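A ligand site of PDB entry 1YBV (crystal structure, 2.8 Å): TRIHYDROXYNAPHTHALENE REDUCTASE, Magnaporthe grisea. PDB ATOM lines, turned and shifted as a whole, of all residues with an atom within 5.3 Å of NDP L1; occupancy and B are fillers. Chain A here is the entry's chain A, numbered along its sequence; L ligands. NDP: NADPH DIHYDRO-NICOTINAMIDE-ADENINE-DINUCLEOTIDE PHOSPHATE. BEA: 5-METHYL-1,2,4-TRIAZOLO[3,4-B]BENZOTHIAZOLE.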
ATOM      1  N   THR A  35      17.534 -19.722  -6.857  1.00  0.00           N
ATOM      2  CA  THR A  35      18.993 -19.712  -6.835  1.00  0.00           C
ATOM      3  C   THR A  35      19.519 -19.432  -8.224  1.00  0.00           C
ATOM      4  O   THR A  35      18.963 -19.909  -9.224  1.00  0.00           O
ATOM      5  CB  THR A  35      19.548 -21.030  -6.324  1.00  0.00           C
ATOM      6  OG1 THR A  35      19.090 -22.091  -7.169  1.00  0.00           O
ATOM      7  CG2 THR A  35      19.093 -21.288  -4.886  1.00  0.00           C
ATOM      8  N   GLY A  36      20.609 -18.677  -8.311  1.00  0.00           N
ATOM      9  CA  GLY A  36      21.174 -18.337  -9.605  1.00  0.00           C
ATOM     10  C   GLY A  36      20.180 -17.580 -10.463  1.00  0.00           C
ATOM     11  O   GLY A  36      19.966 -17.927 -11.603  1.00  0.00           O
ATOM     12  N   ALA A  37      19.602 -16.521  -9.895  1.00  0.00           N
ATOM     13  CA  ALA A  37      18.594 -15.696 -10.586  1.00  0.00           C
ATOM     14  C   ALA A  37      19.082 -14.400 -11.222  1.00  0.00           C
ATOM     15  O   ALA A  37      18.288 -13.547 -11.576  1.00  0.00           O
ATOM     16  CB  ALA A  37      17.433 -15.410  -9.636  1.00  0.00           C
ATOM     17  N   GLY A  38      20.397 -14.238 -11.358  1.00  0.00           N
ATOM     18  CA  GLY A  38      20.921 -13.051 -11.993  1.00  0.00           C
ATOM     19  C   GLY A  38      20.871 -13.126 -13.506  1.00  0.00           C
ATOM     20  O   GLY A  38      20.892 -12.105 -14.198  1.00  0.00           O
ATOM     21  N   ARG A  39      20.811 -14.331 -14.059  1.00  0.00           N
ATOM     22  CA  ARG A  39      20.756 -14.463 -15.507  1.00  0.00           C
ATOM     23  C   ARG A  39      20.151 -15.789 -15.968  1.00  0.00           C
ATOM     24  O   ARG A  39      19.674 -16.585 -15.150  1.00  0.00           O
ATOM     25  CB  ARG A  39      22.146 -14.268 -16.127  1.00  0.00           C
ATOM     26  CG  ARG A  39      23.177 -15.259 -15.647  1.00  0.00           C
ATOM     27  CD  ARG A  39      24.577 -14.703 -15.795  1.00  0.00           C
ATOM     28  NE  ARG A  39      25.572 -15.647 -15.272  1.00  0.00           N
ATOM     29  CZ  ARG A  39      26.129 -16.607 -15.993  1.00  0.00           C
ATOM     30  NH1 ARG A  39      25.801 -16.779 -17.274  1.00  0.00           N
ATOM     31  NH2 ARG A  39      27.005 -17.431 -15.434  1.00  0.00           N
ATOM     32  N   GLY A  40      20.132 -16.000 -17.282  1.00  0.00           N
ATOM     33  CA  GLY A  40      19.605 -17.212 -17.861  1.00  0.00           C
ATOM     34  C   GLY A  40      18.155 -17.518 -17.519  1.00  0.00           C
ATOM     35  O   GLY A  40      17.336 -16.624 -17.364  1.00  0.00           O
ATOM     36  N   ILE A  41      17.860 -18.811 -17.388  1.00  0.00           N
ATOM     37  CA  ILE A  41      16.529 -19.296 -17.063  1.00  0.00           C
ATOM     38  C   ILE A  41      16.084 -18.789 -15.699  1.00  0.00           C
ATOM     39  O   ILE A  41      14.941 -18.396 -15.506  1.00  0.00           O
ATOM     40  CB  ILE A  41      16.505 -20.851 -17.064  1.00  0.00           C
ATOM     41  CG1 ILE A  41      16.902 -21.383 -18.435  1.00  0.00           C
ATOM     42  CG2 ILE A  41      15.138 -21.362 -16.687  1.00  0.00           C
ATOM     43  CD1 ILE A  41      16.974 -22.875 -18.486  1.00  0.00           C
ATOM     44  N   GLY A  42      17.018 -18.782 -14.753  1.00  0.00           N
ATOM     45  CA  GLY A  42      16.714 -18.340 -13.403  1.00  0.00           C
ATOM     46  C   GLY A  42      16.187 -16.933 -13.323  1.00  0.00           C
ATOM     47  O   GLY A  42      15.225 -16.666 -12.600  1.00  0.00           O
ATOM     48  N   ASN A  59      18.882 -15.133  -5.652  1.00  0.00           N
ATOM     49  CA  ASN A  59      20.192 -15.521  -5.155  1.00  0.00           C
ATOM     50  C   ASN A  59      21.160 -15.400  -6.305  1.00  0.00           C
ATOM     51  O   ASN A  59      20.760 -15.460  -7.478  1.00  0.00           O
ATOM     52  CB  ASN A  59      20.171 -16.956  -4.586  1.00  0.00           C
ATOM     53  CG  ASN A  59      21.516 -17.660  -4.696  1.00  0.00           C
ATOM     54  OD1 ASN A  59      21.851 -18.208  -5.750  1.00  0.00           O
ATOM     55  ND2 ASN A  59      22.290 -17.645  -3.631  1.00  0.00           N
ATOM     56  N   TYR A  60      22.425 -15.168  -5.991  1.00  0.00           N
ATOM     57  CA  TYR A  60      23.452 -15.043  -7.001  1.00  0.00           C
ATOM     58  C   TYR A  60      24.773 -15.467  -6.380  1.00  0.00           C
ATOM     59  O   TYR A  60      24.925 -15.475  -5.155  1.00  0.00           O
ATOM     60  CB  TYR A  60      23.536 -13.607  -7.511  1.00  0.00           C
ATOM     61  CG  TYR A  60      23.952 -12.586  -6.481  1.00  0.00           C
ATOM     62  CD1 TYR A  60      23.019 -12.013  -5.625  1.00  0.00           C
ATOM     63  CD2 TYR A  60      25.292 -12.205  -6.342  1.00  0.00           C
ATOM     64  CE1 TYR A  60      23.410 -11.112  -4.648  1.00  0.00           C
ATOM     65  CE2 TYR A  60      25.688 -11.304  -5.372  1.00  0.00           C
ATOM     66  CZ  TYR A  60      24.742 -10.762  -4.535  1.00  0.00           C
ATOM     67  OH  TYR A  60      25.136  -9.897  -3.538  1.00  0.00           O
ATOM     68  N   ALA A  61      25.735 -15.777  -7.246  1.00  0.00           N
ATOM     69  CA  ALA A  61      27.069 -16.184  -6.830  1.00  0.00           C
ATOM     70  C   ALA A  61      28.098 -15.139  -7.218  1.00  0.00           C
ATOM     71  O   ALA A  61      28.926 -14.744  -6.397  1.00  0.00           O
ATOM     72  CB  ALA A  61      27.419 -17.516  -7.468  1.00  0.00           C
ATOM     73  N   ASN A  62      28.060 -14.714  -8.475  1.00  0.00           N
ATOM     74  CA  ASN A  62      29.009 -13.737  -8.987  1.00  0.00           C
ATOM     75  C   ASN A  62      28.366 -12.524  -9.661  1.00  0.00           C
ATOM     76  O   ASN A  62      28.846 -11.403  -9.488  1.00  0.00           O
ATOM     77  CB  ASN A  62      29.955 -14.382  -9.985  1.00  0.00           C
ATOM     78  CG  ASN A  62      30.656 -15.592  -9.419  1.00  0.00           C
ATOM     79  OD1 ASN A  62      30.146 -16.710  -9.490  1.00  0.00           O
ATOM     80  ND2 ASN A  62      31.818 -15.370  -8.807  1.00  0.00           N
ATOM     81  N   SER A  63      27.301 -12.753 -10.413  1.00  0.00           N
ATOM     82  CA  SER A  63      26.608 -11.688 -11.142  1.00  0.00           C
ATOM     83  C   SER A  63      25.843 -10.642 -10.322  1.00  0.00           C
ATOM     84  O   SER A  63      24.673 -10.368 -10.605  1.00  0.00           O
ATOM     85  CB  SER A  63      25.669 -12.328 -12.150  1.00  0.00           C
ATOM     86  OG  SER A  63      26.333 -13.392 -12.805  1.00  0.00           O
ATOM     87  N   ALA A  86      25.217 -16.173  -2.319  1.00  0.00           N
ATOM     88  CA  ALA A  86      25.572 -17.475  -1.768  1.00  0.00           C
ATOM     89  C   ALA A  86      26.098 -18.402  -2.849  1.00  0.00           C
ATOM     90  O   ALA A  86      25.603 -18.390  -3.988  1.00  0.00           O
ATOM     91  CB  ALA A  86      24.371 -18.115  -1.070  1.00  0.00           C
ATOM     92  N   ASN A  87      27.133 -19.158  -2.518  1.00  0.00           N
ATOM     93  CA  ASN A  87      27.719 -20.108  -3.442  1.00  0.00           C
ATOM     94  C   ASN A  87      27.175 -21.474  -3.061  1.00  0.00           C
ATOM     95  O   ASN A  87      27.559 -22.057  -2.043  1.00  0.00           O
ATOM     96  CB  ASN A  87      29.234 -20.127  -3.350  1.00  0.00           C
ATOM     97  CG  ASN A  87      29.856 -21.049  -4.388  1.00  0.00           C
ATOM     98  OD1 ASN A  87      29.663 -22.264  -4.367  1.00  0.00           O
ATOM     99  ND2 ASN A  87      30.578 -20.474  -5.325  1.00  0.00           N
ATOM    100  N   VAL A  88      26.265 -21.975  -3.879  1.00  0.00           N
ATOM    101  CA  VAL A  88      25.641 -23.261  -3.664  1.00  0.00           C
ATOM    102  C   VAL A  88      26.616 -24.427  -3.501  1.00  0.00           C
ATOM    103  O   VAL A  88      26.252 -25.486  -3.002  1.00  0.00           O
ATOM    104  CB  VAL A  88      24.611 -23.494  -4.775  1.00  0.00           C
ATOM    105  CG1 VAL A  88      24.233 -24.952  -4.870  1.00  0.00           C
ATOM    106  CG2 VAL A  88      23.377 -22.648  -4.504  1.00  0.00           C
ATOM    107  N   GLY A  89      27.877 -24.227  -3.892  1.00  0.00           N
ATOM    108  CA  GLY A  89      28.851 -25.290  -3.741  1.00  0.00           C
ATOM    109  C   GLY A  89      29.445 -25.306  -2.344  1.00  0.00           C
ATOM    110  O   GLY A  89      30.313 -26.134  -2.039  1.00  0.00           O
ATOM    111  N   ASN A 114      17.756 -23.615  -9.197  1.00  0.00           N
ATOM    112  CA  ASN A 114      18.123 -23.430 -10.590  1.00  0.00           C
ATOM    113  C   ASN A 114      19.608 -23.545 -10.966  1.00  0.00           C
ATOM    114  O   ASN A 114      19.945 -24.165 -11.974  1.00  0.00           O
ATOM    115  CB  ASN A 114      17.562 -22.084 -11.072  1.00  0.00           C
ATOM    116  CG  ASN A 114      18.047 -21.693 -12.454  1.00  0.00           C
ATOM    117  OD1 ASN A 114      17.709 -22.336 -13.437  1.00  0.00           O
ATOM    118  ND2 ASN A 114      18.832 -20.634 -12.525  1.00  0.00           N
ATOM    119  N   SER A 115      20.474 -22.926 -10.182  1.00  0.00           N
ATOM    120  CA  SER A 115      21.915 -22.911 -10.446  1.00  0.00           C
ATOM    121  C   SER A 115      22.476 -24.234 -10.982  1.00  0.00           C
ATOM    122  O   SER A 115      22.073 -25.311 -10.547  1.00  0.00           O
ATOM    123  CB  SER A 115      22.659 -22.540  -9.174  1.00  0.00           C
ATOM    124  OG  SER A 115      22.082 -21.403  -8.563  1.00  0.00           O
ATOM    125  N   GLY A 116      23.418 -24.132 -11.926  1.00  0.00           N
ATOM    126  CA  GLY A 116      24.027 -25.313 -12.496  1.00  0.00           C
ATOM    127  C   GLY A 116      25.155 -24.962 -13.447  1.00  0.00           C
ATOM    128  O   GLY A 116      25.291 -23.792 -13.814  1.00  0.00           O
ATOM    129  N   VAL A 117      25.973 -25.946 -13.827  1.00  0.00           N
ATOM    130  CA  VAL A 117      27.081 -25.732 -14.751  1.00  0.00           C
ATOM    131  C   VAL A 117      27.167 -26.886 -15.751  1.00  0.00           C
ATOM    132  O   VAL A 117      26.712 -27.981 -15.437  1.00  0.00           O
ATOM    133  CB  VAL A 117      28.436 -25.633 -13.997  1.00  0.00           C
ATOM    134  CG1 VAL A 117      28.387 -24.525 -12.965  1.00  0.00           C
ATOM    135  CG2 VAL A 117      28.800 -26.943 -13.339  1.00  0.00           C
ATOM    136  N   ILE A 137      28.162 -28.593  -7.663  1.00  0.00           N
ATOM    137  CA  ILE A 137      27.147 -27.553  -7.853  1.00  0.00           C
ATOM    138  C   ILE A 137      25.821 -28.182  -8.287  1.00  0.00           C
ATOM    139  O   ILE A 137      24.796 -28.047  -7.593  1.00  0.00           O
ATOM    140  CB  ILE A 137      27.600 -26.514  -8.917  1.00  0.00           C
ATOM    141  CG1 ILE A 137      28.825 -25.757  -8.399  1.00  0.00           C
ATOM    142  CG2 ILE A 137      26.495 -25.523  -9.228  1.00  0.00           C
ATOM    143  CD1 ILE A 137      29.373 -24.761  -9.363  1.00  0.00           C
ATOM    144  N   ASN A 138      25.878 -28.940  -9.380  1.00  0.00           N
ATOM    145  CA  ASN A 138      24.707 -29.602  -9.946  1.00  0.00           C
ATOM    146  C   ASN A 138      23.971 -30.596  -9.067  1.00  0.00           C
ATOM    147  O   ASN A 138      22.752 -30.588  -9.018  1.00  0.00           O
ATOM    148  CB  ASN A 138      25.078 -30.314 -11.252  1.00  0.00           C
ATOM    149  CG  ASN A 138      25.381 -29.365 -12.375  1.00  0.00           C
ATOM    150  OD1 ASN A 138      25.661 -28.184 -12.156  1.00  0.00           O
ATOM    151  ND2 ASN A 138      25.349 -29.874 -13.600  1.00  0.00           N
ATOM    152  N   MET A 162      16.021 -28.274 -10.698  1.00  0.00           N
ATOM    153  CA  MET A 162      16.361 -28.108 -12.096  1.00  0.00           C
ATOM    154  C   MET A 162      17.128 -29.301 -12.624  1.00  0.00           C
ATOM    155  O   MET A 162      18.203 -29.638 -12.117  1.00  0.00           O
ATOM    156  CB  MET A 162      17.161 -26.837 -12.294  1.00  0.00           C
ATOM    157  CG  MET A 162      17.580 -26.574 -13.721  1.00  0.00           C
ATOM    158  SD  MET A 162      16.190 -26.455 -14.861  1.00  0.00           S
ATOM    159  CE  MET A 162      15.547 -24.866 -14.441  1.00  0.00           C
ATOM    160  N   GLY A 163      16.555 -29.965 -13.625  1.00  0.00           N
ATOM    161  CA  GLY A 163      17.176 -31.118 -14.251  1.00  0.00           C
ATOM    162  C   GLY A 163      17.535 -30.774 -15.682  1.00  0.00           C
ATOM    163  O   GLY A 163      17.833 -29.621 -15.992  1.00  0.00           O
ATOM    164  N   SER A 164      17.480 -31.756 -16.568  1.00  0.00           N
ATOM    165  CA  SER A 164      17.806 -31.520 -17.972  1.00  0.00           C
ATOM    166  C   SER A 164      17.392 -32.687 -18.848  1.00  0.00           C
ATOM    167  O   SER A 164      17.259 -33.806 -18.385  1.00  0.00           O
ATOM    168  CB  SER A 164      19.301 -31.289 -18.137  1.00  0.00           C
ATOM    169  OG  SER A 164      19.635 -31.212 -19.503  1.00  0.00           O
ATOM    170  N   ILE A 165      17.243 -32.419 -20.140  1.00  0.00           N
ATOM    171  CA  ILE A 165      16.860 -33.452 -21.096  1.00  0.00           C
ATOM    172  C   ILE A 165      17.959 -34.528 -21.163  1.00  0.00           C
ATOM    173  O   ILE A 165      17.687 -35.706 -21.414  1.00  0.00           O
ATOM    174  CB  ILE A 165      16.613 -32.865 -22.497  1.00  0.00           C
ATOM    175  CG1 ILE A 165      16.086 -33.941 -23.440  1.00  0.00           C
ATOM    176  CG2 ILE A 165      17.886 -32.264 -23.065  1.00  0.00           C
ATOM    177  CD1 ILE A 165      15.716 -33.440 -24.809  1.00  0.00           C
ATOM    178  N   TYR A 178      28.014 -34.340 -16.883  1.00  0.00           N
ATOM    179  CA  TYR A 178      26.887 -33.431 -16.778  1.00  0.00           C
ATOM    180  C   TYR A 178      25.567 -34.213 -16.767  1.00  0.00           C
ATOM    181  O   TYR A 178      24.701 -33.971 -15.922  1.00  0.00           O
ATOM    182  CB  TYR A 178      26.898 -32.432 -17.920  1.00  0.00           C
ATOM    183  CG  TYR A 178      25.727 -31.478 -17.914  1.00  0.00           C
ATOM    184  CD1 TYR A 178      25.640 -30.461 -16.974  1.00  0.00           C
ATOM    185  CD2 TYR A 178      24.713 -31.601 -18.854  1.00  0.00           C
ATOM    186  CE1 TYR A 178      24.570 -29.581 -16.973  1.00  0.00           C
ATOM    187  CE2 TYR A 178      23.643 -30.735 -18.863  1.00  0.00           C
ATOM    188  CZ  TYR A 178      23.580 -29.721 -17.918  1.00  0.00           C
ATOM    189  OH  TYR A 178      22.511 -28.868 -17.938  1.00  0.00           O
ATOM    190  N   LYS A 182      22.535 -34.446 -13.598  1.00  0.00           N
ATOM    191  CA  LYS A 182      21.139 -34.098 -13.805  1.00  0.00           C
ATOM    192  C   LYS A 182      20.258 -35.340 -13.620  1.00  0.00           C
ATOM    193  O   LYS A 182      19.133 -35.250 -13.129  1.00  0.00           O
ATOM    194  CB  LYS A 182      20.959 -33.502 -15.196  1.00  0.00           C
ATOM    195  CG  LYS A 182      21.673 -32.197 -15.386  1.00  0.00           C
ATOM    196  CD  LYS A 182      21.289 -31.216 -14.283  1.00  0.00           C
ATOM    197  CE  LYS A 182      21.599 -29.782 -14.668  1.00  0.00           C
ATOM    198  NZ  LYS A 182      21.134 -28.828 -13.620  1.00  0.00           N
ATOM    199  N   PRO A 208      14.316 -29.137 -18.760  1.00  0.00           N
ATOM    200  CA  PRO A 208      14.363 -28.361 -19.998  1.00  0.00           C
ATOM    201  C   PRO A 208      15.151 -29.099 -21.062  1.00  0.00           C
ATOM    202  O   PRO A 208      15.829 -30.077 -20.776  1.00  0.00           O
ATOM    203  CB  PRO A 208      15.100 -27.095 -19.559  1.00  0.00           C
ATOM    204  CG  PRO A 208      14.729 -26.963 -18.146  1.00  0.00           C
ATOM    205  CD  PRO A 208      14.884 -28.365 -17.652  1.00  0.00           C
ATOM    206  N   GLY A 209      15.125 -28.584 -22.283  1.00  0.00           N
ATOM    207  CA  GLY A 209      15.857 -29.246 -23.335  1.00  0.00           C
ATOM    208  C   GLY A 209      16.490 -28.317 -24.342  1.00  0.00           C
ATOM    209  O   GLY A 209      16.289 -28.501 -25.555  1.00  0.00           O
ATOM    210  N   GLY A 210      17.280 -27.356 -23.890  1.00  0.00           N
ATOM    211  CA  GLY A 210      17.921 -26.468 -24.861  1.00  0.00           C
ATOM    212  C   GLY A 210      17.199 -25.149 -24.911  1.00  0.00           C
ATOM    213  O   GLY A 210      16.278 -24.962 -25.721  1.00  0.00           O
ATOM    214  N   ILE A 211      17.646 -24.232 -24.068  1.00  0.00           N
ATOM    215  CA  ILE A 211      17.062 -22.914 -23.919  1.00  0.00           C
ATOM    216  C   ILE A 211      18.101 -21.846 -24.242  1.00  0.00           C
ATOM    217  O   ILE A 211      19.268 -21.950 -23.821  1.00  0.00           O
ATOM    218  CB  ILE A 211      16.585 -22.722 -22.465  1.00  0.00           C
ATOM    219  CG1 ILE A 211      15.664 -23.867 -22.036  1.00  0.00           C
ATOM    220  CG2 ILE A 211      15.933 -21.372 -22.294  1.00  0.00           C
ATOM    221  CD1 ILE A 211      14.356 -23.959 -22.807  1.00  0.00           C
ATOM    222  N   THR A 213      20.175 -19.123 -23.623  1.00  0.00           N
ATOM    223  CA  THR A 213      20.700 -18.408 -22.489  1.00  0.00           C
ATOM    224  C   THR A 213      22.200 -18.311 -22.744  1.00  0.00           C
ATOM    225  O   THR A 213      22.678 -18.712 -23.825  1.00  0.00           O
ATOM    226  CB  THR A 213      20.444 -19.175 -21.155  1.00  0.00           C
ATOM    227  OG1 THR A 213      21.129 -20.431 -21.189  1.00  0.00           O
ATOM    228  CG2 THR A 213      18.971 -19.444 -20.958  1.00  0.00           C
ATOM    229  N   ASP A 214      22.961 -17.764 -21.791  1.00  0.00           N
ATOM    230  CA  ASP A 214      24.416 -17.658 -21.945  1.00  0.00           C
ATOM    231  C   ASP A 214      24.979 -19.051 -22.186  1.00  0.00           C
ATOM    232  O   ASP A 214      25.824 -19.224 -23.067  1.00  0.00           O
ATOM    233  CB  ASP A 214      25.063 -17.057 -20.684  1.00  0.00           C
ATOM    234  CG  ASP A 214      24.619 -15.617 -20.424  1.00  0.00           C
ATOM    235  OD1 ASP A 214      24.302 -14.889 -21.410  1.00  0.00           O
ATOM    236  OD2 ASP A 214      24.582 -15.211 -19.236  1.00  0.00           O
ATOM    237  N   MET A 215      24.487 -20.032 -21.431  1.00  0.00           N
ATOM    238  CA  MET A 215      24.946 -21.422 -21.574  1.00  0.00           C
ATOM    239  C   MET A 215      24.762 -21.875 -23.015  1.00  0.00           C
ATOM    240  O   MET A 215      25.694 -22.406 -23.628  1.00  0.00           O
ATOM    241  CB  MET A 215      24.165 -22.360 -20.648  1.00  0.00           C
ATOM    242  CG  MET A 215      24.735 -23.770 -20.598  1.00  0.00           C
ATOM    243  SD  MET A 215      23.807 -24.924 -19.553  1.00  0.00           S
ATOM    244  CE  MET A 215      24.411 -24.458 -17.923  1.00  0.00           C
ATOM    245  N   TYR A 216      23.585 -21.628 -23.559  1.00  0.00           N
ATOM    246  CA  TYR A 216      23.270 -22.007 -24.929  1.00  0.00           C
ATOM    247  C   TYR A 216      24.290 -21.392 -25.879  1.00  0.00           C
ATOM    248  O   TYR A 216      24.813 -22.076 -26.757  1.00  0.00           O
ATOM    249  CB  TYR A 216      21.856 -21.538 -25.288  1.00  0.00           C
ATOM    250  CG  TYR A 216      21.417 -21.823 -26.710  1.00  0.00           C
ATOM    251  CD1 TYR A 216      21.653 -20.912 -27.728  1.00  0.00           C
ATOM    252  CD2 TYR A 216      20.683 -22.978 -26.999  1.00  0.00           C
ATOM    253  CE1 TYR A 216      21.146 -21.122 -29.022  1.00  0.00           C
ATOM    254  CE2 TYR A 216      20.188 -23.204 -28.282  1.00  0.00           C
ATOM    255  CZ  TYR A 216      20.425 -22.278 -29.290  1.00  0.00           C
ATOM    256  OH  TYR A 216      19.880 -22.473 -30.538  1.00  0.00           O
HETATM  257  PA  NDP L   1      23.730 -19.873 -17.238  1.00  0.00           P
HETATM  258  O1A NDP L   1      25.004 -20.414 -17.777  1.00  0.00           O
HETATM  259  O2A NDP L   1      23.066 -18.739 -17.942  1.00  0.00           O
HETATM  260  O5B NDP L   1      24.001 -19.543 -15.671  1.00  0.00           O
HETATM  261  C5B NDP L   1      22.869 -19.573 -14.761  1.00  0.00           C
HETATM  262  C4B NDP L   1      23.205 -19.386 -13.328  1.00  0.00           C
HETATM  263  O4B NDP L   1      23.714 -20.442 -12.521  1.00  0.00           O
HETATM  264  C3B NDP L   1      23.785 -18.105 -12.817  1.00  0.00           C
HETATM  265  O3B NDP L   1      23.159 -17.279 -12.056  1.00  0.00           O
HETATM  266  C2B NDP L   1      25.023 -18.564 -12.067  1.00  0.00           C
HETATM  267  O2B NDP L   1      25.320 -17.634 -10.987  1.00  0.00           O
HETATM  268  C1B NDP L   1      24.568 -19.898 -11.513  1.00  0.00           C
HETATM  269  N9A NDP L   1      25.472 -20.540 -10.734  1.00  0.00           N
HETATM  270  C8A NDP L   1      26.580 -21.177 -11.133  1.00  0.00           C
HETATM  271  N7A NDP L   1      27.317 -21.505 -10.066  1.00  0.00           N
HETATM  272  C5A NDP L   1      26.642 -21.050  -9.035  1.00  0.00           C
HETATM  273  C6A NDP L   1      26.972 -21.216  -7.699  1.00  0.00           C
HETATM  274  N6A NDP L   1      28.137 -21.726  -7.305  1.00  0.00           N
HETATM  275  N1A NDP L   1      26.072 -20.742  -6.807  1.00  0.00           N
HETATM  276  C2A NDP L   1      24.951 -20.129  -7.183  1.00  0.00           C
HETATM  277  N3A NDP L   1      24.653 -19.962  -8.471  1.00  0.00           N
HETATM  278  C4A NDP L   1      25.481 -20.427  -9.415  1.00  0.00           C
HETATM  279  O3  NDP L   1      22.674 -21.083 -17.121  1.00  0.00           O
HETATM  280  PN  NDP L   1      21.160 -21.384 -17.594  1.00  0.00           P
HETATM  281  O1N NDP L   1      20.382 -20.234 -17.056  1.00  0.00           O
HETATM  282  O2N NDP L   1      21.182 -21.720 -19.036  1.00  0.00           O
HETATM  283  O5D NDP L   1      20.844 -22.750 -16.801  1.00  0.00           O
HETATM  284  C5D NDP L   1      20.240 -22.692 -15.509  1.00  0.00           C
HETATM  285  C4D NDP L   1      19.918 -24.096 -15.049  1.00  0.00           C
HETATM  286  O4D NDP L   1      19.089 -24.805 -15.982  1.00  0.00           O
HETATM  287  C3D NDP L   1      21.178 -24.914 -14.896  1.00  0.00           C
HETATM  288  O3D NDP L   1      21.052 -25.771 -13.755  1.00  0.00           O
HETATM  289  C2D NDP L   1      21.255 -25.698 -16.194  1.00  0.00           C
HETATM  290  O2D NDP L   1      22.042 -26.879 -16.065  1.00  0.00           O
HETATM  291  C1D NDP L   1      19.805 -25.983 -16.387  1.00  0.00           C
HETATM  292  N1N NDP L   1      19.543 -26.235 -17.809  1.00  0.00           N
HETATM  293  C2N NDP L   1      19.836 -25.281 -18.805  1.00  0.00           C
HETATM  294  C3N NDP L   1      19.507 -25.544 -20.138  1.00  0.00           C
HETATM  295  C7N NDP L   1      19.927 -24.657 -21.318  1.00  0.00           C
HETATM  296  O7N NDP L   1      19.868 -25.084 -22.461  1.00  0.00           O
HETATM  297  N7N NDP L   1      20.411 -23.440 -21.043  1.00  0.00           N
HETATM  298  C4N NDP L   1      18.872 -26.749 -20.424  1.00  0.00           C
HETATM  299  C5N NDP L   1      18.590 -27.691 -19.435  1.00  0.00           C
HETATM  300  C6N NDP L   1      18.928 -27.438 -18.107  1.00  0.00           C
HETATM  301  P2B NDP L   1      26.377 -16.434 -11.176  1.00  0.00           P
HETATM  302  O1X NDP L   1      25.833 -15.431 -10.254  1.00  0.00           O
HETATM  303  O2X NDP L   1      26.255 -16.087 -12.620  1.00  0.00           O
HETATM  304  O3X NDP L   1      27.640 -17.097 -10.729  1.00  0.00           O
HETATM  305  C1  BEA L   2      22.239 -26.473 -24.262  1.00  0.00           C
HETATM  306  C2  BEA L   2      23.037 -25.526 -23.368  1.00  0.00           C
HETATM  307  C3  BEA L   2      22.109 -26.219 -25.650  1.00  0.00           C
HETATM  308  C4  BEA L   2      21.382 -27.071 -26.504  1.00  0.00           C
HETATM  309  C5  BEA L   2      20.763 -28.216 -26.006  1.00  0.00           C
HETATM  310  C6  BEA L   2      20.885 -28.474 -24.622  1.00  0.00           C
HETATM  311  C7  BEA L   2      20.886 -29.220 -22.338  1.00  0.00           C
HETATM  312  C8  BEA L   2      21.596 -27.629 -23.779  1.00  0.00           C
HETATM  313  C9  BEA L   2      22.026 -27.835 -21.350  1.00  0.00           C
HETATM  314  N1  BEA L   2      21.547 -28.142 -22.525  1.00  0.00           N
HETATM  315  N2  BEA L   2      21.658 -28.655 -20.450  1.00  0.00           N
HETATM  316  N3  BEA L   2      20.885 -29.632 -21.148  1.00  0.00           N
HETATM  317  S   BEA L   2      20.149 -29.881 -23.829  1.00  0.00           S
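OD1 of Asn 87 sits at hydrogen-bond distance from N of Gly 89, at 2.7 Å.
The side-chain amide nitrogen of Asn 59 sits close to the backbone carbonyl oxygen of Ala 86, at 3.4 Å.
The backbone NH (N) of Gly 42 sits close to the side-chain amide nitrogen (ND2) of Asn 114 (3.4 Å).
OG of Ser 115 sits at hydrogen-bond distance from N of Gly 36 (3.1 Å).
The backbone NH (N) of Ala 86 sits at hydrogen-bond distance from the backbone carbonyl oxygen (O) of Tyr 60, 2.9 Å away.
The side-chain hydroxyl of Ser 63 is in hydrogen-bond range of the guanidinium group of Arg 39 (3.4 Å).
The backbone carbonyl oxygen (O) of Gly 36 is in hydrogen-bond range of the side-chain amide nitrogen (ND2) of Asn 114 (3.1 Å).
The backbone NH (N) of Ile 165 sits at hydrogen-bond distance from the backbone carbonyl oxygen (O) of Pro 208, at 2.8 Å.
The side-chain sulfur of Met 162 lies close to an oxygen (O4D) of NDP L1.
Merely in contact with NDP L1: Gly 40, Gly 163, Gly 210, Met 215, Pro 208, Ser 164, Ala 86, Asp 214, Ile 137 and Asn 59.
Hydrophobic or aromatic side chains that line NDP L1: Ile 41, Ala 61, Val 88, Ile 137, Met 162, Tyr 178, Pro 208 and Met 215.
Of the 37 residues printed, 26 come within 4 Å of NDP L1.
The backbone NH (N) of Ser 63 is in hydrogen-bond range of an oxygen (O1X) of NDP L1.
An oxygen (O1X) of NDP L1 sits at hydrogen-bond distance from the backbone NH (N) of Ala 61, at 3.0 Å.
The side-chain amide oxygen (OD1) of Asn 62 lies close to an oxygen (O3X) of NDP L1, at 2.8 Å.
O7N of NDP L1 sits at hydrogen-bond distance from N of Ile 211 (2.9 Å).
The side-chain hydroxyl of Tyr 178 lies within hydrogen-bond range of an oxygen (O2D) of NDP L1 (2.8 Å).
The backbone NH (N) of Gly 116 sits close to an oxygen (O3D) of NDP L1.
An oxygen (O2X) of NDP L1 is in hydrogen-bond range of the side-chain hydroxyl (OG) of Ser 63, at 2.7 Å.
The backbone carbonyl oxygen (O) of Asn 114 is in hydrogen-bond range of an oxygen (O3D) of NDP L1, at 2.6 Å.
N1A of NDP L1 is in hydrogen-bond range of N of Val 88 (3.2 Å).
The side-chain hydroxyl (OH) of Tyr 178 sits at hydrogen-bond distance from a nitrogen (N2) of BEA L2 (2.7 Å).
The side-chain hydroxyl (OG) of Ser 115 sits at hydrogen-bond distance from a nitrogen (N3A) of NDP L1 (2.9 Å).
The backbone NH (N) of Ile 41 sits at hydrogen-bond distance from an oxygen (O1N) of NDP L1, 2.9 Å away.
OG1 of Thr 213 is in hydrogen-bond range of O2N of NDP L1.
NE of Arg 39 is in salt-bridge range of O2X of NDP L1 (2.8 Å).
O of Gly 36 is in hydrogen-bond range of O3B of NDP L1, at 3.3 Å.
The side-chain amino group (NZ) of Lys 182 is in hydrogen-bond range of an oxygen (O3D) of NDP L1, at 3.1 Å.
O3D of NDP L1 is in hydrogen-bond range of O of Ser 115.
N7N of NDP L1 sits at hydrogen-bond distance from O of Ile 211, at 3.4 Å.
N3 of BEA L2 is in hydrogen-bond range of OG of Ser 164.
O1X of NDP L1 lies within hydrogen-bond range of N of Asn 62, at 2.9 Å.
The side-chain amide oxygen (OD1) of Asn 87 lies within hydrogen-bond range of a nitrogen (N6A) of NDP L1 (3.4 Å).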
